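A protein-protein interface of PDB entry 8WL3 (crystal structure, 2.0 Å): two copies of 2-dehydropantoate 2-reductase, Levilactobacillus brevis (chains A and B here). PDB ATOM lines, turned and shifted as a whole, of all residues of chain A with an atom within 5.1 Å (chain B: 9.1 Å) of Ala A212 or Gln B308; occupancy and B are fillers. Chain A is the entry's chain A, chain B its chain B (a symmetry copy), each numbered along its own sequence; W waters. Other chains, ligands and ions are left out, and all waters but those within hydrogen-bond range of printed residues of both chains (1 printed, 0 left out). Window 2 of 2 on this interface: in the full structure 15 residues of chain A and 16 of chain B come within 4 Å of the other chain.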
ATOM      1  N   GLY A 208      11.615  -3.344  31.412  1.00  0.00           N
ATOM      2  CA  GLY A 208      10.478  -3.398  30.500  1.00  0.00           C
ATOM      3  C   GLY A 208      10.603  -2.443  29.317  1.00  0.00           C
ATOM      4  O   GLY A 208      10.273  -2.782  28.165  1.00  0.00           O
ATOM      5  N   GLU A 209      11.094  -1.243  29.591  1.00  0.00           N
ATOM      6  CA  GLU A 209      11.308  -0.269  28.513  1.00  0.00           C
ATOM      7  C   GLU A 209      12.353  -0.762  27.513  1.00  0.00           C
ATOM      8  O   GLU A 209      12.189  -0.572  26.299  1.00  0.00           O
ATOM      9  CB  GLU A 209      11.681   1.083  29.076  1.00  0.00           C
ATOM     10  CG  GLU A 209      10.520   1.755  29.799  1.00  0.00           C
ATOM     11  CD  GLU A 209      10.941   2.958  30.635  1.00  0.00           C
ATOM     12  OE1 GLU A 209      10.116   3.870  30.847  1.00  0.00           O
ATOM     13  OE2 GLU A 209      12.090   2.990  31.110  1.00  0.00           O
ATOM     14  N   PHE A 210      13.393  -1.417  28.015  1.00  0.00           N
ATOM     15  CA  PHE A 210      14.396  -2.021  27.136  1.00  0.00           C
ATOM     16  C   PHE A 210      13.726  -3.075  26.248  1.00  0.00           C
ATOM     17  O   PHE A 210      13.886  -3.073  25.017  1.00  0.00           O
ATOM     18  CB  PHE A 210      15.548  -2.650  27.933  1.00  0.00           C
ATOM     19  CG  PHE A 210      16.555  -3.364  27.069  1.00  0.00           C
ATOM     20  CD1 PHE A 210      17.480  -2.657  26.315  1.00  0.00           C
ATOM     21  CD2 PHE A 210      16.533  -4.739  26.964  1.00  0.00           C
ATOM     22  CE1 PHE A 210      18.381  -3.312  25.498  1.00  0.00           C
ATOM     23  CE2 PHE A 210      17.413  -5.402  26.143  1.00  0.00           C
ATOM     24  CZ  PHE A 210      18.352  -4.699  25.420  1.00  0.00           C
ATOM     25  N   GLY A 211      12.957  -3.956  26.883  1.00  0.00           N
ATOM     26  CA  GLY A 211      12.253  -5.007  26.139  1.00  0.00           C
ATOM     27  C   GLY A 211      11.213  -4.539  25.137  1.00  0.00           C
ATOM     28  O   GLY A 211      10.848  -5.286  24.238  1.00  0.00           O
ATOM     29  N   ALA A 212      10.735  -3.310  25.300  1.00  0.00           N
ATOM     30  CA  ALA A 212       9.769  -2.705  24.374  1.00  0.00           C
ATOM     31  C   ALA A 212      10.436  -2.044  23.166  1.00  0.00           C
ATOM     32  O   ALA A 212       9.753  -1.609  22.230  1.00  0.00           O
ATOM     33  CB  ALA A 212       8.900  -1.695  25.124  1.00  0.00           C
ATOM     34  N   LEU A 213      11.763  -1.952  23.185  1.00  0.00           N
ATOM     35  CA  LEU A 213      12.501  -1.367  22.074  1.00  0.00           C
ATOM     36  C   LEU A 213      12.377  -2.220  20.827  1.00  0.00           C
ATOM     37  O   LEU A 213      12.503  -3.428  20.880  1.00  0.00           O
ATOM     38  CB  LEU A 213      14.001  -1.204  22.408  1.00  0.00           C
ATOM     39  CG  LEU A 213      14.331  -0.158  23.472  1.00  0.00           C
ATOM     40  CD1 LEU A 213      15.786  -0.232  23.868  1.00  0.00           C
ATOM     41  CD2 LEU A 213      13.999   1.248  22.996  1.00  0.00           C
ATOM     42  N   LYS A 214      12.219  -1.560  19.693  1.00  0.00           N
ATOM     43  CA  LYS A 214      12.044  -2.258  18.433  1.00  0.00           C
ATOM     44  C   LYS A 214      13.326  -2.911  17.961  1.00  0.00           C
ATOM     45  O   LYS A 214      13.290  -3.819  17.121  1.00  0.00           O
ATOM     46  CB  LYS A 214      11.429  -1.311  17.401  1.00  0.00           C
ATOM     47  CG  LYS A 214      10.008  -0.959  17.846  1.00  0.00           C
ATOM     48  CD  LYS A 214       9.248  -0.008  16.941  1.00  0.00           C
ATOM     49  CE  LYS A 214       9.599   1.458  17.143  1.00  0.00           C
ATOM     50  NZ  LYS A 214      10.370   1.977  15.977  1.00  0.00           N
ATOM     51  N   ASN A 215      14.450  -2.497  18.541  1.00  0.00           N
ATOM     52  CA  ASN A 215      15.732  -3.082  18.212  1.00  0.00           C
ATOM     53  C   ASN A 215      16.386  -3.815  19.404  1.00  0.00           C
ATOM     54  O   ASN A 215      17.626  -3.981  19.463  1.00  0.00           O
ATOM     55  CB  ASN A 215      16.643  -1.973  17.661  1.00  0.00           C
ATOM     56  CG  ASN A 215      16.947  -0.889  18.684  1.00  0.00           C
ATOM     57  OD1 ASN A 215      16.270  -0.748  19.701  1.00  0.00           O
ATOM     58  ND2 ASN A 215      17.972  -0.115  18.416  1.00  0.00           N
ATOM     59  N   MET B 267      16.907  15.713  19.590  1.00  0.00           N
ATOM     60  CA  MET B 267      16.497  14.725  20.576  1.00  0.00           C
ATOM     61  C   MET B 267      15.668  15.378  21.651  1.00  0.00           C
ATOM     62  O   MET B 267      14.636  14.835  22.045  1.00  0.00           O
ATOM     63  CB  MET B 267      17.689  14.003  21.217  1.00  0.00           C
ATOM     64  CG  MET B 267      17.326  12.813  22.103  1.00  0.00           C
ATOM     65  SD  MET B 267      16.641  11.376  21.236  1.00  0.00           S
ATOM     66  CE  MET B 267      18.024  10.761  20.327  1.00  0.00           C
ATOM     67  N   GLN B 270      12.084  15.903  20.768  1.00  0.00           N
ATOM     68  CA  GLN B 270      11.430  14.703  20.241  1.00  0.00           C
ATOM     69  C   GLN B 270      11.343  14.655  18.723  1.00  0.00           C
ATOM     70  O   GLN B 270      10.452  14.005  18.192  1.00  0.00           O
ATOM     71  CB  GLN B 270      10.022  14.533  20.810  1.00  0.00           C
ATOM     72  CG  GLN B 270       9.914  14.736  22.300  1.00  0.00           C
ATOM     73  CD  GLN B 270       8.541  14.325  22.825  1.00  0.00           C
ATOM     74  OE1 GLN B 270       7.835  13.508  22.215  1.00  0.00           O
ATOM     75  NE2 GLN B 270       8.159  14.892  23.961  1.00  0.00           N
ATOM     76  N   ARG B 271      12.255  15.331  18.031  1.00  0.00           N
ATOM     77  CA  ARG B 271      12.330  15.263  16.571  1.00  0.00           C
ATOM     78  C   ARG B 271      13.217  14.080  16.168  1.00  0.00           C
ATOM     79  O   ARG B 271      14.197  13.771  16.860  1.00  0.00           O
ATOM     80  CB  ARG B 271      12.903  16.554  15.984  1.00  0.00           C
ATOM     81  CG  ARG B 271      12.007  17.787  16.118  1.00  0.00           C
ATOM     82  CD  ARG B 271      12.519  18.975  15.292  1.00  0.00           C
ATOM     83  NE  ARG B 271      13.886  19.406  15.674  1.00  0.00           N
ATOM     84  CZ  ARG B 271      14.202  20.392  16.527  1.00  0.00           C
ATOM     85  NH1 ARG B 271      13.268  21.106  17.139  1.00  0.00           N
ATOM     86  NH2 ARG B 271      15.473  20.665  16.782  1.00  0.00           N
ATOM     87  N   PRO B 272      12.864  13.386  15.074  1.00  0.00           N
ATOM     88  CA  PRO B 272      13.761  12.320  14.594  1.00  0.00           C
ATOM     89  C   PRO B 272      15.102  12.904  14.175  1.00  0.00           C
ATOM     90  O   PRO B 272      15.144  13.939  13.540  1.00  0.00           O
ATOM     91  CB  PRO B 272      13.013  11.740  13.385  1.00  0.00           C
ATOM     92  CG  PRO B 272      11.576  12.050  13.643  1.00  0.00           C
ATOM     93  CD  PRO B 272      11.558  13.365  14.392  1.00  0.00           C
ATOM     94  N   THR B 273      16.194  12.242  14.533  1.00  0.00           N
ATOM     95  CA  THR B 273      17.533  12.757  14.252  1.00  0.00           C
ATOM     96  C   THR B 273      17.993  12.374  12.858  1.00  0.00           C
ATOM     97  O   THR B 273      17.370  11.522  12.198  1.00  0.00           O
ATOM     98  CB  THR B 273      18.576  12.201  15.234  1.00  0.00           C
ATOM     99  OG1 THR B 273      18.866  10.815  14.927  1.00  0.00           O
ATOM    100  CG2 THR B 273      18.100  12.397  16.681  1.00  0.00           C
ATOM    101  N   GLN B 301      22.173   2.322  16.372  1.00  0.00           N
ATOM    102  CA  GLN B 301      21.128   1.632  17.104  1.00  0.00           C
ATOM    103  C   GLN B 301      20.805   2.316  18.436  1.00  0.00           C
ATOM    104  O   GLN B 301      19.620   2.438  18.812  1.00  0.00           O
ATOM    105  CB  GLN B 301      21.523   0.176  17.351  1.00  0.00           C
ATOM    106  CG  GLN B 301      21.589  -0.679  16.096  1.00  0.00           C
ATOM    107  CD  GLN B 301      20.244  -0.784  15.396  1.00  0.00           C
ATOM    108  OE1 GLN B 301      19.215  -0.914  16.042  1.00  0.00           O
ATOM    109  NE2 GLN B 301      20.248  -0.707  14.063  1.00  0.00           N
ATOM    110  N   LEU B 302      21.847   2.772  19.127  1.00  0.00           N
ATOM    111  CA  LEU B 302      21.683   3.428  20.422  1.00  0.00           C
ATOM    112  C   LEU B 302      20.876   4.701  20.271  1.00  0.00           C
ATOM    113  O   LEU B 302      20.003   4.994  21.092  1.00  0.00           O
ATOM    114  CB  LEU B 302      23.043   3.729  21.079  1.00  0.00           C
ATOM    115  CG  LEU B 302      24.000   2.571  21.399  1.00  0.00           C
ATOM    116  CD1 LEU B 302      25.333   3.100  21.935  1.00  0.00           C
ATOM    117  CD2 LEU B 302      23.375   1.570  22.370  1.00  0.00           C
ATOM    118  N   ILE B 303      21.177   5.462  19.218  1.00  0.00           N
ATOM    119  CA  ILE B 303      20.441   6.697  18.932  1.00  0.00           C
ATOM    120  C   ILE B 303      18.964   6.409  18.596  1.00  0.00           C
ATOM    121  O   ILE B 303      18.063   7.075  19.118  1.00  0.00           O
ATOM    122  CB  ILE B 303      21.114   7.525  17.813  1.00  0.00           C
ATOM    123  CG1 ILE B 303      22.414   8.171  18.311  1.00  0.00           C
ATOM    124  CG2 ILE B 303      20.184   8.634  17.320  1.00  0.00           C
ATOM    125  CD1 ILE B 303      22.267   9.228  19.401  1.00  0.00           C
ATOM    126  N   HIS B 304      18.714   5.421  17.733  1.00  0.00           N
ATOM    127  CA  HIS B 304      17.338   4.983  17.464  1.00  0.00           C
ATOM    128  C   HIS B 304      16.566   4.579  18.742  1.00  0.00           C
ATOM    129  O   HIS B 304      15.400   4.963  18.907  1.00  0.00           O
ATOM    130  CB  HIS B 304      17.327   3.861  16.416  1.00  0.00           C
ATOM    131  CG  HIS B 304      17.594   4.347  15.026  1.00  0.00           C
ATOM    132  ND1 HIS B 304      17.021   5.498  14.527  1.00  0.00           N
ATOM    133  CD2 HIS B 304      18.351   3.842  14.024  1.00  0.00           C
ATOM    134  CE1 HIS B 304      17.437   5.699  13.289  1.00  0.00           C
ATOM    135  NE2 HIS B 304      18.241   4.702  12.956  1.00  0.00           N
ATOM    136  N   SER B 305      17.218   3.870  19.669  1.00  0.00           N
ATOM    137  CA  SER B 305      16.568   3.497  20.920  1.00  0.00           C
ATOM    138  C   SER B 305      16.248   4.713  21.760  1.00  0.00           C
ATOM    139  O   SER B 305      15.177   4.813  22.364  1.00  0.00           O
ATOM    140  CB  SER B 305      17.445   2.541  21.720  1.00  0.00           C
ATOM    141  OG  SER B 305      17.647   1.341  21.008  1.00  0.00           O
ATOM    142  N   GLN B 306      17.201   5.633  21.835  1.00  0.00           N
ATOM    143  CA  GLN B 306      17.002   6.866  22.584  1.00  0.00           C
ATOM    144  C   GLN B 306      15.800   7.649  22.006  1.00  0.00           C
ATOM    145  O   GLN B 306      14.968   8.164  22.747  1.00  0.00           O
ATOM    146  CB  GLN B 306      18.296   7.696  22.540  1.00  0.00           C
ATOM    147  CG  GLN B 306      18.433   8.770  23.597  1.00  0.00           C
ATOM    148  CD  GLN B 306      19.729   9.564  23.422  1.00  0.00           C
ATOM    149  OE1 GLN B 306      20.702   9.071  22.826  1.00  0.00           O
ATOM    150  NE2 GLN B 306      19.746  10.790  23.917  1.00  0.00           N
ATOM    151  N   GLU B 307      15.705   7.727  20.675  1.00  0.00           N
ATOM    152  CA  GLU B 307      14.570   8.406  20.018  1.00  0.00           C
ATOM    153  C   GLU B 307      13.262   7.748  20.428  1.00  0.00           C
ATOM    154  O   GLU B 307      12.301   8.435  20.774  1.00  0.00           O
ATOM    155  CB  GLU B 307      14.653   8.332  18.498  1.00  0.00           C
ATOM    156  CG  GLU B 307      15.704   9.212  17.868  1.00  0.00           C
ATOM    157  CD  GLU B 307      15.721   9.092  16.359  1.00  0.00           C
ATOM    158  OE1 GLU B 307      14.719   8.662  15.793  1.00  0.00           O
ATOM    159  OE2 GLU B 307      16.714   9.466  15.729  1.00  0.00           O
ATOM    160  N   GLN B 308      13.226   6.419  20.400  1.00  0.00           N
ATOM    161  CA  GLN B 308      12.004   5.727  20.778  1.00  0.00           C
ATOM    162  C   GLN B 308      11.590   5.988  22.234  1.00  0.00           C
ATOM    163  O   GLN B 308      10.396   6.204  22.510  1.00  0.00           O
ATOM    164  CB  GLN B 308      12.107   4.243  20.501  1.00  0.00           C
ATOM    165  CG  GLN B 308      10.785   3.505  20.657  1.00  0.00           C
ATOM    166  CD  GLN B 308      10.970   2.007  20.653  1.00  0.00           C
ATOM    167  OE1 GLN B 308      11.865   1.485  19.992  1.00  0.00           O
ATOM    168  NE2 GLN B 308      10.128   1.305  21.416  1.00  0.00           N
ATOM    169  N   LEU B 309      12.552   5.991  23.148  1.00  0.00           N
ATOM    170  CA  LEU B 309      12.272   6.273  24.556  1.00  0.00           C
ATOM    171  C   LEU B 309      11.819   7.703  24.811  1.00  0.00           C
ATOM    172  O   LEU B 309      10.983   7.950  25.671  1.00  0.00           O
ATOM    173  CB  LEU B 309      13.491   5.989  25.419  1.00  0.00           C
ATOM    174  CG  LEU B 309      13.856   4.501  25.418  1.00  0.00           C
ATOM    175  CD1 LEU B 309      15.203   4.297  26.090  1.00  0.00           C
ATOM    176  CD2 LEU B 309      12.776   3.656  26.086  1.00  0.00           C
ATOM    177  N   LYS B 310      12.361   8.630  24.044  1.00  0.00           N
ATOM    178  CA  LYS B 310      12.046  10.035  24.187  1.00  0.00           C
ATOM    179  C   LYS B 310      10.607  10.390  23.819  1.00  0.00           C
ATOM    180  O   LYS B 310      10.133  11.465  24.177  1.00  0.00           O
ATOM    181  CB  LYS B 310      13.005  10.856  23.330  1.00  0.00           C
ATOM    182  CG  LYS B 310      12.999  12.342  23.595  1.00  0.00           C
ATOM    183  CD  LYS B 310      13.489  12.681  24.988  1.00  0.00           C
ATOM    184  CE  LYS B 310      13.333  14.170  25.242  1.00  0.00           C
ATOM    185  NZ  LYS B 310      14.099  14.560  26.458  1.00  0.00           N
ATOM    186  N   GLN B 311       9.915   9.512  23.105  1.00  0.00           N
ATOM    187  CA  GLN B 311       8.508   9.752  22.791  1.00  0.00           C
ATOM    188  C   GLN B 311       7.531   8.897  23.611  1.00  0.00           C
ATOM    189  O   GLN B 311       6.419   8.625  23.168  1.00  0.00           O
ATOM    190  CB  GLN B 311       8.270   9.582  21.291  1.00  0.00           C
ATOM    191  CG  GLN B 311       8.246   8.145  20.814  1.00  0.00           C
ATOM    192  CD  GLN B 311       8.700   8.014  19.378  1.00  0.00           C
ATOM    193  OE1 GLN B 311       9.082   9.000  18.739  1.00  0.00           O
ATOM    194  NE2 GLN B 311       8.680   6.788  18.868  1.00  0.00           N
ATOM    195  N   ILE B 312       7.930   8.503  24.823  1.00  0.00           N
ATOM    196  CA  ILE B 312       7.021   7.819  25.755  1.00  0.00           C
ATOM    197  C   ILE B 312       6.137   8.826  26.496  1.00  0.00           C
ATOM    198  O   ILE B 312       6.363  10.029  26.426  1.00  0.00           O
ATOM    199  CB  ILE B 312       7.779   6.933  26.776  1.00  0.00           C
ATOM    200  CG1 ILE B 312       8.395   5.709  26.063  1.00  0.00           C
ATOM    201  CG2 ILE B 312       6.842   6.493  27.905  1.00  0.00           C
ATOM    202  CD1 ILE B 312       9.364   4.903  26.913  1.00  0.00           C
HETATM  203  O   HOH W   1      14.287   1.467  19.203  1.00  0.00           O
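Gln B308 touches just these residues of chain A: Ala A212 (3.0 Å), Leu A213 (3.6 Å) and Lys A214 (3.1 Å).
No residue of chain B comes within 4 Å of Gly A211.
Printed residues of chain B within 4 Å of Leu A213: Ser B305 (3.8 Å) and Gln B308 (3.6 Å).
Of the printed residues of chain A, Ser B305 touches Leu A213 (3.8 Å) and Asn A215 (2.8 Å).
Of the printed residues of chain B, Asn A215 touches Gln B301 and Ser B305.
Of the printed residues of chain B, Lys A214 touches Gln B308 (3.1 Å).
Printed residues of chain A within 4 Å of Gln B301: Asn A215.
Gln B270 touches none of the printed residues of chain A.
Glu B307 touches none of the printed residues of chain A.
The nearest printed residue of chain B that does not touch Asn A215 is His B304 (4.5 Å).
Ser B305 touches Leu A213 (OG to CD1, 3.8 Å).
Leu A213 touches Gln B308.
Water W1 bridges OE1 of Gln B308 (2.5 Å) and OD1 of Asn A215 (3.0 Å).
Of the 17 printed residues of chain B, 3 touch a printed residue of chain A.
Among the printed residues, 6 pairs touch across the chains.
Among the printed residues, no Asp or Glu carboxylate lies within 4 Å of a Lys or Arg side-chain nitrogen of the other chain.
No position is printed for both chains.
O of Ala A212 sits at hydrogen-bond distance from NE2 of Gln B308, 3.0 Å away.
The backbone NH (N) of Lys A214 lies within hydrogen-bond range of the side-chain amide oxygen (OE1) of Gln B308, at 3.1 Å.
The side-chain amide oxygen of Gln B301 sits at hydrogen-bond distance from the side-chain amide nitrogen of Asn A215 (2.8 Å).
OG of Ser B305 sits at hydrogen-bond distance from OD1 of Asn A215, at 2.8 Å.
The backbone carbonyl oxygen (O) of Gln B301 is in hydrogen-bond range of the side-chain hydroxyl (OG) of Ser B305, 3.1 Å away.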
